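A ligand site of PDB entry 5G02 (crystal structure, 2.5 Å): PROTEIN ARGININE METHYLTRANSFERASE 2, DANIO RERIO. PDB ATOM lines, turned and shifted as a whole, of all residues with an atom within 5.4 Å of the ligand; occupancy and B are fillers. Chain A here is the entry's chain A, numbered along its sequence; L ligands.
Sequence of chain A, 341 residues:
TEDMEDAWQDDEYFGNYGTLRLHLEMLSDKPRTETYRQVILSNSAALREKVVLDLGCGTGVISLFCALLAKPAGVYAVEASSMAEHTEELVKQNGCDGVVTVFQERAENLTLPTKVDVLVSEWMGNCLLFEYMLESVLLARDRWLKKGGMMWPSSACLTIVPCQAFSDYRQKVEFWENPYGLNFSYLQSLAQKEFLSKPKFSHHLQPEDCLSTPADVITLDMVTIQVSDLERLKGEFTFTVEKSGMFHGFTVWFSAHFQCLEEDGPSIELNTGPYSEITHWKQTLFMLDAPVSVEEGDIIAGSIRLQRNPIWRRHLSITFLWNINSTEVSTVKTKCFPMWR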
ATOM      1  N   TYR A  13     -30.634 -21.559  -3.697  1.00  0.00           N
ATOM      2  CA  TYR A  13     -30.358 -22.920  -3.279  1.00  0.00           C
ATOM      3  C   TYR A  13     -30.897 -23.167  -1.880  1.00  0.00           C
ATOM      4  O   TYR A  13     -31.723 -24.059  -1.671  1.00  0.00           O
ATOM      5  CB  TYR A  13     -28.856 -23.203  -3.357  1.00  0.00           C
ATOM      6  CG  TYR A  13     -28.445 -24.571  -2.906  1.00  0.00           C
ATOM      7  CD1 TYR A  13     -28.563 -25.680  -3.750  1.00  0.00           C
ATOM      8  CD2 TYR A  13     -27.893 -24.757  -1.644  1.00  0.00           C
ATOM      9  CE1 TYR A  13     -28.166 -26.955  -3.315  1.00  0.00           C
ATOM     10  CE2 TYR A  13     -27.484 -26.022  -1.201  1.00  0.00           C
ATOM     11  CZ  TYR A  13     -27.623 -27.113  -2.037  1.00  0.00           C
ATOM     12  OH  TYR A  13     -27.207 -28.352  -1.586  1.00  0.00           O
ATOM     13  N   PHE A  14     -30.468 -22.343  -0.916  1.00  0.00           N
ATOM     14  CA  PHE A  14     -30.881 -22.520   0.473  1.00  0.00           C
ATOM     15  C   PHE A  14     -32.320 -22.079   0.727  1.00  0.00           C
ATOM     16  O   PHE A  14     -32.929 -22.515   1.712  1.00  0.00           O
ATOM     17  CB  PHE A  14     -29.934 -21.766   1.430  1.00  0.00           C
ATOM     18  CG  PHE A  14     -28.519 -22.318   1.429  1.00  0.00           C
ATOM     19  CD1 PHE A  14     -28.246 -23.572   1.971  1.00  0.00           C
ATOM     20  CD2 PHE A  14     -27.468 -21.585   0.908  1.00  0.00           C
ATOM     21  CE1 PHE A  14     -26.963 -24.081   1.963  1.00  0.00           C
ATOM     22  CE2 PHE A  14     -26.185 -22.093   0.900  1.00  0.00           C
ATOM     23  CZ  PHE A  14     -25.938 -23.337   1.429  1.00  0.00           C
ATOM     24  N   TYR A  17     -34.512 -25.066   0.291  1.00  0.00           N
ATOM     25  CA  TYR A  17     -34.427 -26.019   1.386  1.00  0.00           C
ATOM     26  C   TYR A  17     -35.075 -25.513   2.660  1.00  0.00           C
ATOM     27  O   TYR A  17     -35.228 -26.296   3.606  1.00  0.00           O
ATOM     28  CB  TYR A  17     -32.967 -26.377   1.655  1.00  0.00           C
ATOM     29  CG  TYR A  17     -32.491 -27.446   0.710  1.00  0.00           C
ATOM     30  CD1 TYR A  17     -33.071 -28.702   0.713  1.00  0.00           C
ATOM     31  CD2 TYR A  17     -31.479 -27.188  -0.209  1.00  0.00           C
ATOM     32  CE1 TYR A  17     -32.656 -29.693  -0.162  1.00  0.00           C
ATOM     33  CE2 TYR A  17     -31.040 -28.184  -1.088  1.00  0.00           C
ATOM     34  CZ  TYR A  17     -31.646 -29.430  -1.048  1.00  0.00           C
ATOM     35  OH  TYR A  17     -31.241 -30.437  -1.891  1.00  0.00           O
ATOM     36  N   HIS A  23     -37.755 -31.374   1.499  1.00  0.00           N
ATOM     37  CA  HIS A  23     -37.582 -32.347   2.564  1.00  0.00           C
ATOM     38  C   HIS A  23     -38.608 -33.457   2.464  1.00  0.00           C
ATOM     39  O   HIS A  23     -38.298 -34.619   2.757  1.00  0.00           O
ATOM     40  CB  HIS A  23     -37.656 -31.663   3.923  1.00  0.00           C
ATOM     41  CG  HIS A  23     -36.542 -30.690   4.145  1.00  0.00           C
ATOM     42  ND1 HIS A  23     -35.250 -31.082   4.390  1.00  0.00           N
ATOM     43  CD2 HIS A  23     -36.532 -29.339   4.108  1.00  0.00           C
ATOM     44  CE1 HIS A  23     -34.482 -30.023   4.520  1.00  0.00           C
ATOM     45  NE2 HIS A  23     -35.240 -28.945   4.352  1.00  0.00           N
ATOM     46  N   MET A  26     -37.267 -35.901   0.089  1.00  0.00           N
ATOM     47  CA  MET A  26     -36.104 -36.660   0.542  1.00  0.00           C
ATOM     48  C   MET A  26     -36.494 -37.753   1.525  1.00  0.00           C
ATOM     49  O   MET A  26     -36.003 -38.882   1.416  1.00  0.00           O
ATOM     50  CB  MET A  26     -35.068 -35.719   1.173  1.00  0.00           C
ATOM     51  CG  MET A  26     -34.482 -34.783   0.165  1.00  0.00           C
ATOM     52  SD  MET A  26     -33.149 -33.750   0.770  1.00  0.00           S
ATOM     53  CE  MET A  26     -31.946 -34.229  -0.483  1.00  0.00           C
ATOM     54  N   LEU A  27     -37.364 -37.442   2.481  1.00  0.00           N
ATOM     55  CA  LEU A  27     -37.812 -38.444   3.439  1.00  0.00           C
ATOM     56  C   LEU A  27     -38.790 -39.427   2.825  1.00  0.00           C
ATOM     57  O   LEU A  27     -38.964 -40.529   3.369  1.00  0.00           O
ATOM     58  CB  LEU A  27     -38.437 -37.749   4.653  1.00  0.00           C
ATOM     59  CG  LEU A  27     -37.488 -36.744   5.321  1.00  0.00           C
ATOM     60  CD1 LEU A  27     -38.242 -35.804   6.247  1.00  0.00           C
ATOM     61  CD2 LEU A  27     -36.389 -37.483   6.077  1.00  0.00           C
ATOM     62  N   ARG A  32     -33.214 -44.145  -0.105  1.00  0.00           N
ATOM     63  CA  ARG A  32     -32.195 -43.178   0.285  1.00  0.00           C
ATOM     64  C   ARG A  32     -32.124 -43.030   1.799  1.00  0.00           C
ATOM     65  O   ARG A  32     -31.040 -43.102   2.386  1.00  0.00           O
ATOM     66  CB  ARG A  32     -32.494 -41.817  -0.358  1.00  0.00           C
ATOM     67  CG  ARG A  32     -31.619 -40.647   0.111  1.00  0.00           C
ATOM     68  CD  ARG A  32     -32.338 -39.333  -0.159  1.00  0.00           C
ATOM     69  NE  ARG A  32     -33.059 -38.952   1.062  1.00  0.00           N
ATOM     70  CZ  ARG A  32     -32.564 -38.217   2.063  1.00  0.00           C
ATOM     71  NH1 ARG A  32     -31.387 -37.646   1.956  1.00  0.00           N
ATOM     72  NH2 ARG A  32     -33.317 -37.997   3.141  1.00  0.00           N
ATOM     73  N   ASP A  54     -22.929 -34.172  11.132  1.00  0.00           N
ATOM     74  CA  ASP A  54     -23.960 -34.348  10.099  1.00  0.00           C
ATOM     75  C   ASP A  54     -23.999 -33.062   9.267  1.00  0.00           C
ATOM     76  O   ASP A  54     -24.647 -32.068   9.641  1.00  0.00           O
ATOM     77  CB  ASP A  54     -25.318 -34.663  10.730  1.00  0.00           C
ATOM     78  CG  ASP A  54     -26.448 -34.852   9.698  1.00  0.00           C
ATOM     79  OD1 ASP A  54     -26.244 -34.644   8.477  1.00  0.00           O
ATOM     80  OD2 ASP A  54     -27.566 -35.207  10.110  1.00  0.00           O
ATOM     81  N   LEU A  55     -23.339 -33.082   8.108  1.00  0.00           N
ATOM     82  CA  LEU A  55     -23.179 -31.891   7.295  1.00  0.00           C
ATOM     83  C   LEU A  55     -24.389 -31.700   6.383  1.00  0.00           C
ATOM     84  O   LEU A  55     -24.589 -32.477   5.446  1.00  0.00           O
ATOM     85  CB  LEU A  55     -21.903 -31.957   6.463  1.00  0.00           C
ATOM     86  CG  LEU A  55     -21.684 -30.545   5.940  1.00  0.00           C
ATOM     87  CD1 LEU A  55     -20.663 -29.888   6.807  1.00  0.00           C
ATOM     88  CD2 LEU A  55     -21.273 -30.482   4.481  1.00  0.00           C
ATOM     89  N   GLY A  56     -25.154 -30.639   6.615  1.00  0.00           N
ATOM     90  CA  GLY A  56     -26.346 -30.388   5.838  1.00  0.00           C
ATOM     91  C   GLY A  56     -27.466 -31.282   6.318  1.00  0.00           C
ATOM     92  O   GLY A  56     -28.064 -32.014   5.514  1.00  0.00           O
ATOM     93  N   CYS A  57     -27.762 -31.217   7.618  1.00  0.00           N
ATOM     94  CA  CYS A  57     -28.665 -32.165   8.264  1.00  0.00           C
ATOM     95  C   CYS A  57     -30.133 -31.996   7.852  1.00  0.00           C
ATOM     96  O   CYS A  57     -30.920 -32.918   8.053  1.00  0.00           O
ATOM     97  CB  CYS A  57     -28.553 -32.029   9.783  1.00  0.00           C
ATOM     98  SG  CYS A  57     -29.108 -30.446  10.440  1.00  0.00           S
ATOM     99  N   GLY A  58     -30.505 -30.852   7.278  1.00  0.00           N
ATOM    100  CA  GLY A  58     -31.884 -30.661   6.869  1.00  0.00           C
ATOM    101  C   GLY A  58     -32.828 -30.705   8.049  1.00  0.00           C
ATOM    102  O   GLY A  58     -32.646 -29.965   9.018  1.00  0.00           O
ATOM    103  N   THR A  59     -33.824 -31.600   7.994  1.00  0.00           N
ATOM    104  CA  THR A  59     -34.708 -31.838   9.133  1.00  0.00           C
ATOM    105  C   THR A  59     -34.000 -32.483  10.319  1.00  0.00           C
ATOM    106  O   THR A  59     -34.582 -32.524  11.412  1.00  0.00           O
ATOM    107  CB  THR A  59     -35.859 -32.737   8.707  1.00  0.00           C
ATOM    108  OG1 THR A  59     -35.336 -33.792   7.897  1.00  0.00           O
ATOM    109  CG2 THR A  59     -36.884 -31.951   7.910  1.00  0.00           C
ATOM    110  N   VAL A  61     -32.664 -35.785  10.204  1.00  0.00           N
ATOM    111  CA  VAL A  61     -33.024 -37.203  10.274  1.00  0.00           C
ATOM    112  C   VAL A  61     -31.806 -38.072  10.567  1.00  0.00           C
ATOM    113  O   VAL A  61     -31.854 -38.979  11.410  1.00  0.00           O
ATOM    114  CB  VAL A  61     -33.735 -37.623   8.982  1.00  0.00           C
ATOM    115  CG1 VAL A  61     -32.889 -37.264   7.779  1.00  0.00           C
ATOM    116  CG2 VAL A  61     -34.065 -39.091   8.995  1.00  0.00           C
ATOM    117  N   ILE A  62     -30.694 -37.820   9.881  1.00  0.00           N
ATOM    118  CA  ILE A  62     -29.472 -38.609  10.084  1.00  0.00           C
ATOM    119  C   ILE A  62     -28.945 -38.404  11.507  1.00  0.00           C
ATOM    120  O   ILE A  62     -28.444 -39.340  12.138  1.00  0.00           O
ATOM    121  CB  ILE A  62     -28.413 -38.263   9.019  1.00  0.00           C
ATOM    122  CG1 ILE A  62     -29.000 -38.372   7.605  1.00  0.00           C
ATOM    123  CG2 ILE A  62     -27.169 -39.147   9.144  1.00  0.00           C
ATOM    124  CD1 ILE A  62     -27.992 -38.005   6.515  1.00  0.00           C
ATOM    125  N   VAL A  78     -25.501 -29.536  11.164  1.00  0.00           N
ATOM    126  CA  VAL A  78     -25.165 -28.262  10.550  1.00  0.00           C
ATOM    127  C   VAL A  78     -26.097 -28.019   9.368  1.00  0.00           C
ATOM    128  O   VAL A  78     -26.110 -28.799   8.410  1.00  0.00           O
ATOM    129  CB  VAL A  78     -23.695 -28.233  10.110  1.00  0.00           C
ATOM    130  CG1 VAL A  78     -23.417 -26.970   9.309  1.00  0.00           C
ATOM    131  CG2 VAL A  78     -22.815 -28.262  11.334  1.00  0.00           C
ATOM    132  N   GLU A  79     -26.844 -26.921   9.420  1.00  0.00           N
ATOM    133  CA  GLU A  79     -27.794 -26.618   8.352  1.00  0.00           C
ATOM    134  C   GLU A  79     -27.809 -25.117   8.100  1.00  0.00           C
ATOM    135  O   GLU A  79     -28.115 -24.334   9.014  1.00  0.00           O
ATOM    136  CB  GLU A  79     -29.205 -27.125   8.733  1.00  0.00           C
ATOM    137  CG  GLU A  79     -30.300 -26.734   7.748  1.00  0.00           C
ATOM    138  CD  GLU A  79     -30.013 -27.224   6.352  1.00  0.00           C
ATOM    139  OE1 GLU A  79     -29.651 -28.417   6.187  1.00  0.00           O
ATOM    140  OE2 GLU A  79     -30.095 -26.399   5.417  1.00  0.00           O
ATOM    141  N   ALA A  80     -27.518 -24.712   6.863  1.00  0.00           N
ATOM    142  CA  ALA A  80     -27.462 -23.297   6.536  1.00  0.00           C
ATOM    143  C   ALA A  80     -28.827 -22.673   6.268  1.00  0.00           C
ATOM    144  O   ALA A  80     -28.968 -21.454   6.362  1.00  0.00           O
ATOM    145  CB  ALA A  80     -26.541 -23.084   5.324  1.00  0.00           C
ATOM    146  N   SER A  81     -29.839 -23.469   5.935  1.00  0.00           N
ATOM    147  CA  SER A  81     -31.121 -22.874   5.593  1.00  0.00           C
ATOM    148  C   SER A  81     -31.934 -22.576   6.839  1.00  0.00           C
ATOM    149  O   SER A  81     -31.608 -22.994   7.954  1.00  0.00           O
ATOM    150  CB  SER A  81     -31.922 -23.789   4.663  1.00  0.00           C
ATOM    151  OG  SER A  81     -32.538 -24.824   5.401  1.00  0.00           O
ATOM    152  N   GLU A 105     -25.401 -22.615  10.198  1.00  0.00           N
ATOM    153  CA  GLU A 105     -24.203 -22.071   9.578  1.00  0.00           C
ATOM    154  C   GLU A 105     -23.936 -22.804   8.268  1.00  0.00           C
ATOM    155  O   GLU A 105     -24.388 -23.928   8.062  1.00  0.00           O
ATOM    156  CB  GLU A 105     -22.974 -22.177  10.498  1.00  0.00           C
ATOM    157  CG  GLU A 105     -23.122 -21.493  11.865  1.00  0.00           C
ATOM    158  CD  GLU A 105     -21.920 -21.680  12.797  1.00  0.00           C
ATOM    159  OE1 GLU A 105     -20.862 -22.160  12.345  1.00  0.00           O
ATOM    160  OE2 GLU A 105     -22.047 -21.351  13.991  1.00  0.00           O
ATOM    161  N   ARG A 106     -23.211 -22.145   7.376  1.00  0.00           N
ATOM    162  CA  ARG A 106     -22.684 -22.810   6.196  1.00  0.00           C
ATOM    163  C   ARG A 106     -21.443 -23.606   6.579  1.00  0.00           C
ATOM    164  O   ARG A 106     -20.666 -23.188   7.433  1.00  0.00           O
ATOM    165  CB  ARG A 106     -22.340 -21.785   5.103  1.00  0.00           C
ATOM    166  CG  ARG A 106     -23.324 -21.801   3.961  1.00  0.00           C
ATOM    167  CD  ARG A 106     -23.235 -20.548   3.103  1.00  0.00           C
ATOM    168  NE  ARG A 106     -22.171 -20.624   2.114  1.00  0.00           N
ATOM    169  CZ  ARG A 106     -21.043 -19.942   2.204  1.00  0.00           C
ATOM    170  NH1 ARG A 106     -20.839 -19.128   3.239  1.00  0.00           N
ATOM    171  NH2 ARG A 106     -20.119 -20.068   1.268  1.00  0.00           N
ATOM    172  N   ALA A 107     -21.273 -24.759   5.933  1.00  0.00           N
ATOM    173  CA  ALA A 107     -20.069 -25.559   6.141  1.00  0.00           C
ATOM    174  C   ALA A 107     -18.809 -24.732   5.953  1.00  0.00           C
ATOM    175  O   ALA A 107     -17.822 -24.919   6.670  1.00  0.00           O
ATOM    176  CB  ALA A 107     -20.056 -26.735   5.161  1.00  0.00           C
ATOM    177  N   GLU A 108     -18.844 -23.795   5.014  1.00  0.00           N
ATOM    178  CA  GLU A 108     -17.648 -23.048   4.647  1.00  0.00           C
ATOM    179  C   GLU A 108     -17.154 -22.169   5.794  1.00  0.00           C
ATOM    180  O   GLU A 108     -15.976 -22.192   6.148  1.00  0.00           O
ATOM    181  CB  GLU A 108     -17.947 -22.221   3.398  1.00  0.00           C
ATOM    182  CG  GLU A 108     -18.060 -23.066   2.122  1.00  0.00           C
ATOM    183  CD  GLU A 108     -19.457 -23.650   1.861  1.00  0.00           C
ATOM    184  OE1 GLU A 108     -20.296 -23.679   2.784  1.00  0.00           O
ATOM    185  OE2 GLU A 108     -19.726 -24.084   0.718  1.00  0.00           O
ATOM    186  N   GLU A 122     -25.493 -36.295   3.230  1.00  0.00           N
ATOM    187  CA  GLU A 122     -26.189 -36.741   2.031  1.00  0.00           C
ATOM    188  C   GLU A 122     -26.121 -35.566   1.051  1.00  0.00           C
ATOM    189  O   GLU A 122     -26.979 -34.684   1.054  1.00  0.00           O
ATOM    190  CB  GLU A 122     -27.626 -37.188   2.319  1.00  0.00           C
ATOM    191  CG  GLU A 122     -28.275 -37.976   1.176  1.00  0.00           C
ATOM    192  CD  GLU A 122     -28.755 -37.062   0.039  1.00  0.00           C
ATOM    193  OE1 GLU A 122     -29.786 -36.385   0.205  1.00  0.00           O
ATOM    194  OE2 GLU A 122     -28.101 -37.035  -1.018  1.00  0.00           O
ATOM    195  N   TRP A 123     -25.080 -35.566   0.225  1.00  0.00           N
ATOM    196  CA  TRP A 123     -24.734 -34.451  -0.647  1.00  0.00           C
ATOM    197  C   TRP A 123     -24.956 -34.730  -2.128  1.00  0.00           C
ATOM    198  O   TRP A 123     -24.744 -33.826  -2.947  1.00  0.00           O
ATOM    199  CB  TRP A 123     -23.272 -34.053  -0.432  1.00  0.00           C
ATOM    200  CG  TRP A 123     -22.327 -35.216  -0.608  1.00  0.00           C
ATOM    201  CD1 TRP A 123     -21.824 -36.013   0.383  1.00  0.00           C
ATOM    202  CD2 TRP A 123     -21.790 -35.720  -1.845  1.00  0.00           C
ATOM    203  NE1 TRP A 123     -21.006 -36.984  -0.155  1.00  0.00           N
ATOM    204  CE2 TRP A 123     -20.961 -36.813  -1.518  1.00  0.00           C
ATOM    205  CE3 TRP A 123     -21.912 -35.346  -3.183  1.00  0.00           C
ATOM    206  CZ2 TRP A 123     -20.270 -37.549  -2.484  1.00  0.00           C
ATOM    207  CZ3 TRP A 123     -21.231 -36.073  -4.144  1.00  0.00           C
ATOM    208  CH2 TRP A 123     -20.426 -37.161  -3.788  1.00  0.00           C
ATOM    209  N   MET A 133     -22.535 -29.600  -3.899  1.00  0.00           N
ATOM    210  CA  MET A 133     -22.482 -29.681  -2.442  1.00  0.00           C
ATOM    211  C   MET A 133     -21.276 -30.482  -1.990  1.00  0.00           C
ATOM    212  O   MET A 133     -20.786 -30.281  -0.865  1.00  0.00           O
ATOM    213  CB  MET A 133     -23.771 -30.290  -1.858  1.00  0.00           C
ATOM    214  CG  MET A 133     -23.791 -30.351  -0.332  1.00  0.00           C
ATOM    215  SD  MET A 133     -25.301 -31.035   0.405  1.00  0.00           S
ATOM    216  CE  MET A 133     -24.772 -31.260   2.104  1.00  0.00           C
ATOM    217  N   SER A 136     -18.593 -28.206  -0.440  1.00  0.00           N
ATOM    218  CA  SER A 136     -18.786 -27.923   0.978  1.00  0.00           C
ATOM    219  C   SER A 136     -18.336 -29.099   1.833  1.00  0.00           C
ATOM    220  O   SER A 136     -17.625 -28.920   2.823  1.00  0.00           O
ATOM    221  CB  SER A 136     -20.248 -27.598   1.256  1.00  0.00           C
ATOM    222  OG  SER A 136     -20.806 -26.817   0.216  1.00  0.00           O
ATOM    223  N   ARG A 314     -22.578 -23.802  -9.269  1.00  0.00           N
ATOM    224  CA  ARG A 314     -23.440 -24.935  -8.991  1.00  0.00           C
ATOM    225  C   ARG A 314     -23.769 -25.727 -10.237  1.00  0.00           C
ATOM    226  O   ARG A 314     -24.533 -26.701 -10.155  1.00  0.00           O
ATOM    227  CB  ARG A 314     -24.714 -24.470  -8.293  1.00  0.00           C
ATOM    228  CG  ARG A 314     -24.393 -24.032  -6.860  1.00  0.00           C
ATOM    229  CD  ARG A 314     -25.530 -24.293  -5.904  1.00  0.00           C
ATOM    230  NE  ARG A 314     -25.265 -23.697  -4.589  1.00  0.00           N
ATOM    231  CZ  ARG A 314     -24.887 -24.377  -3.507  1.00  0.00           C
ATOM    232  NH1 ARG A 314     -24.716 -25.690  -3.545  1.00  0.00           N
ATOM    233  NH2 ARG A 314     -24.704 -23.734  -2.375  1.00  0.00           N
HETATM  234  N1  LIG L   1     -29.596 -34.829   5.525  1.00  0.00           N
HETATM  235  C1  LIG L   1     -30.897 -34.221   5.109  1.00  0.00           C
HETATM  236  C2  LIG L   1     -31.835 -35.260   4.833  1.00  0.00           C
HETATM  237  O1  LIG L   1     -31.397 -36.459   4.528  1.00  0.00           O
HETATM  238  O2  LIG L   1     -33.147 -35.063   4.885  1.00  0.00           O
HETATM  239  C3  LIG L   1     -30.766 -33.322   3.886  1.00  0.00           C
HETATM  240  C4  LIG L   1     -29.518 -33.468   2.994  1.00  0.00           C
HETATM  241  C5  LIG L   1     -29.643 -32.697   1.780  1.00  0.00           C
HETATM  242  N2  LIG L   1     -29.251 -33.501   0.641  1.00  0.00           N
HETATM  243  C6  LIG L   1     -28.763 -31.432   1.699  1.00  0.00           C
HETATM  244  C7  LIG L   1     -28.932 -30.444   2.821  1.00  0.00           C
HETATM  245  O3  LIG L   1     -27.623 -29.864   3.066  1.00  0.00           O
HETATM  246  C8  LIG L   1     -29.836 -29.345   2.536  1.00  0.00           C
HETATM  247  O4  LIG L   1     -30.763 -29.161   3.578  1.00  0.00           O
HETATM  248  C9  LIG L   1     -28.966 -28.144   2.372  1.00  0.00           C
HETATM  249  O5  LIG L   1     -29.561 -27.007   2.881  1.00  0.00           O
HETATM  250  C10 LIG L   1     -27.783 -28.464   3.157  1.00  0.00           C
HETATM  251  N3  LIG L   1     -26.599 -27.870   2.708  1.00  0.00           N
HETATM  252  C11 LIG L   1     -26.084 -27.874   1.472  1.00  0.00           C
HETATM  253  N4  LIG L   1     -24.937 -27.204   1.489  1.00  0.00           N
HETATM  254  C12 LIG L   1     -24.721 -26.786   2.755  1.00  0.00           C
HETATM  255  C13 LIG L   1     -23.691 -26.065   3.385  1.00  0.00           C
HETATM  256  N5  LIG L   1     -22.563 -25.584   2.634  1.00  0.00           N
HETATM  257  N6  LIG L   1     -23.764 -25.816   4.693  1.00  0.00           N
HETATM  258  C14 LIG L   1     -24.820 -26.244   5.411  1.00  0.00           C
HETATM  259  N7  LIG L   1     -25.807 -26.934   4.842  1.00  0.00           N
HETATM  260  C15 LIG L   1     -25.784 -27.217   3.535  1.00  0.00           C
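The side-chain sulfur (SD) of Met 133 sits close to an oxygen (O3) of the ligand (3.7 Å). Merely in contact with the ligand: Met 26, Tyr 13, Arg 106, Glu 105, Phe 14, Tyr 17, Val 61, Ile 62, Gly 58, His 23 and Thr 59.
The side-chain carboxylate (OE1) of Glu 108 lies within salt-bridge range of the guanidinium group (NE) of Arg 106 (3.6 Å). The backbone NH (N) of Glu 105 lies within hydrogen-bond range of the backbone carbonyl oxygen (O) of Glu 79, 3.4 Å away. The backbone carbonyl oxygen (O) of Val 78 lies within hydrogen-bond range of the backbone NH (N) of Cys 57 (3.0 Å). The side-chain carboxylate (OE1) of Glu 79 lies within hydrogen-bond range of the backbone NH (N) of Gly 58. N of Gly 56 lies within hydrogen-bond range of O of Val 78 (2.7 Å). NE2 of His 23 is in hydrogen-bond range of O of Tyr 17 (2.8 Å). The guanidinium group (NE) of Arg 32 lies within hydrogen-bond range of the backbone carbonyl oxygen (O) of Met 26, 3.0 Å away. N of Ala 80 sits at hydrogen-bond distance from O of Glu 105, at 3.4 Å.
The backbone carbonyl oxygen (O) of Glu 122 lies within hydrogen-bond range of a nitrogen (N2) of the ligand (2.6 Å). A nitrogen (N6) of the ligand sits at hydrogen-bond distance from the backbone NH (N) of Ala 107 (3.0 Å). O of Gly 56 is in hydrogen-bond range of N1 of the ligand. The side-chain hydroxyl (OG) of Ser 136 is in hydrogen-bond range of a nitrogen (N5) of the ligand (3.2 Å). The side-chain carboxylate (OE1) of Glu 122 is in salt-bridge range of a nitrogen (N2) of the ligand (3.0 Å). The backbone carbonyl oxygen (O) of Cys 57 sits close to a nitrogen (N1) of the ligand (3.4 Å). OE1 of Glu 108 lies within hydrogen-bond range of N5 of the ligand (3.0 Å). The side-chain carboxylate of Glu 79 sits at hydrogen-bond distance from an oxygen (O5) of the ligand (2.7 Å). A nitrogen (N7) of the ligand lies close to the backbone NH (N) of Ala 80, at 3.5 Å. The guanidinium group of Arg 32 lies within salt-bridge range of an oxygen (O1) of the ligand, at 2.8 Å.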
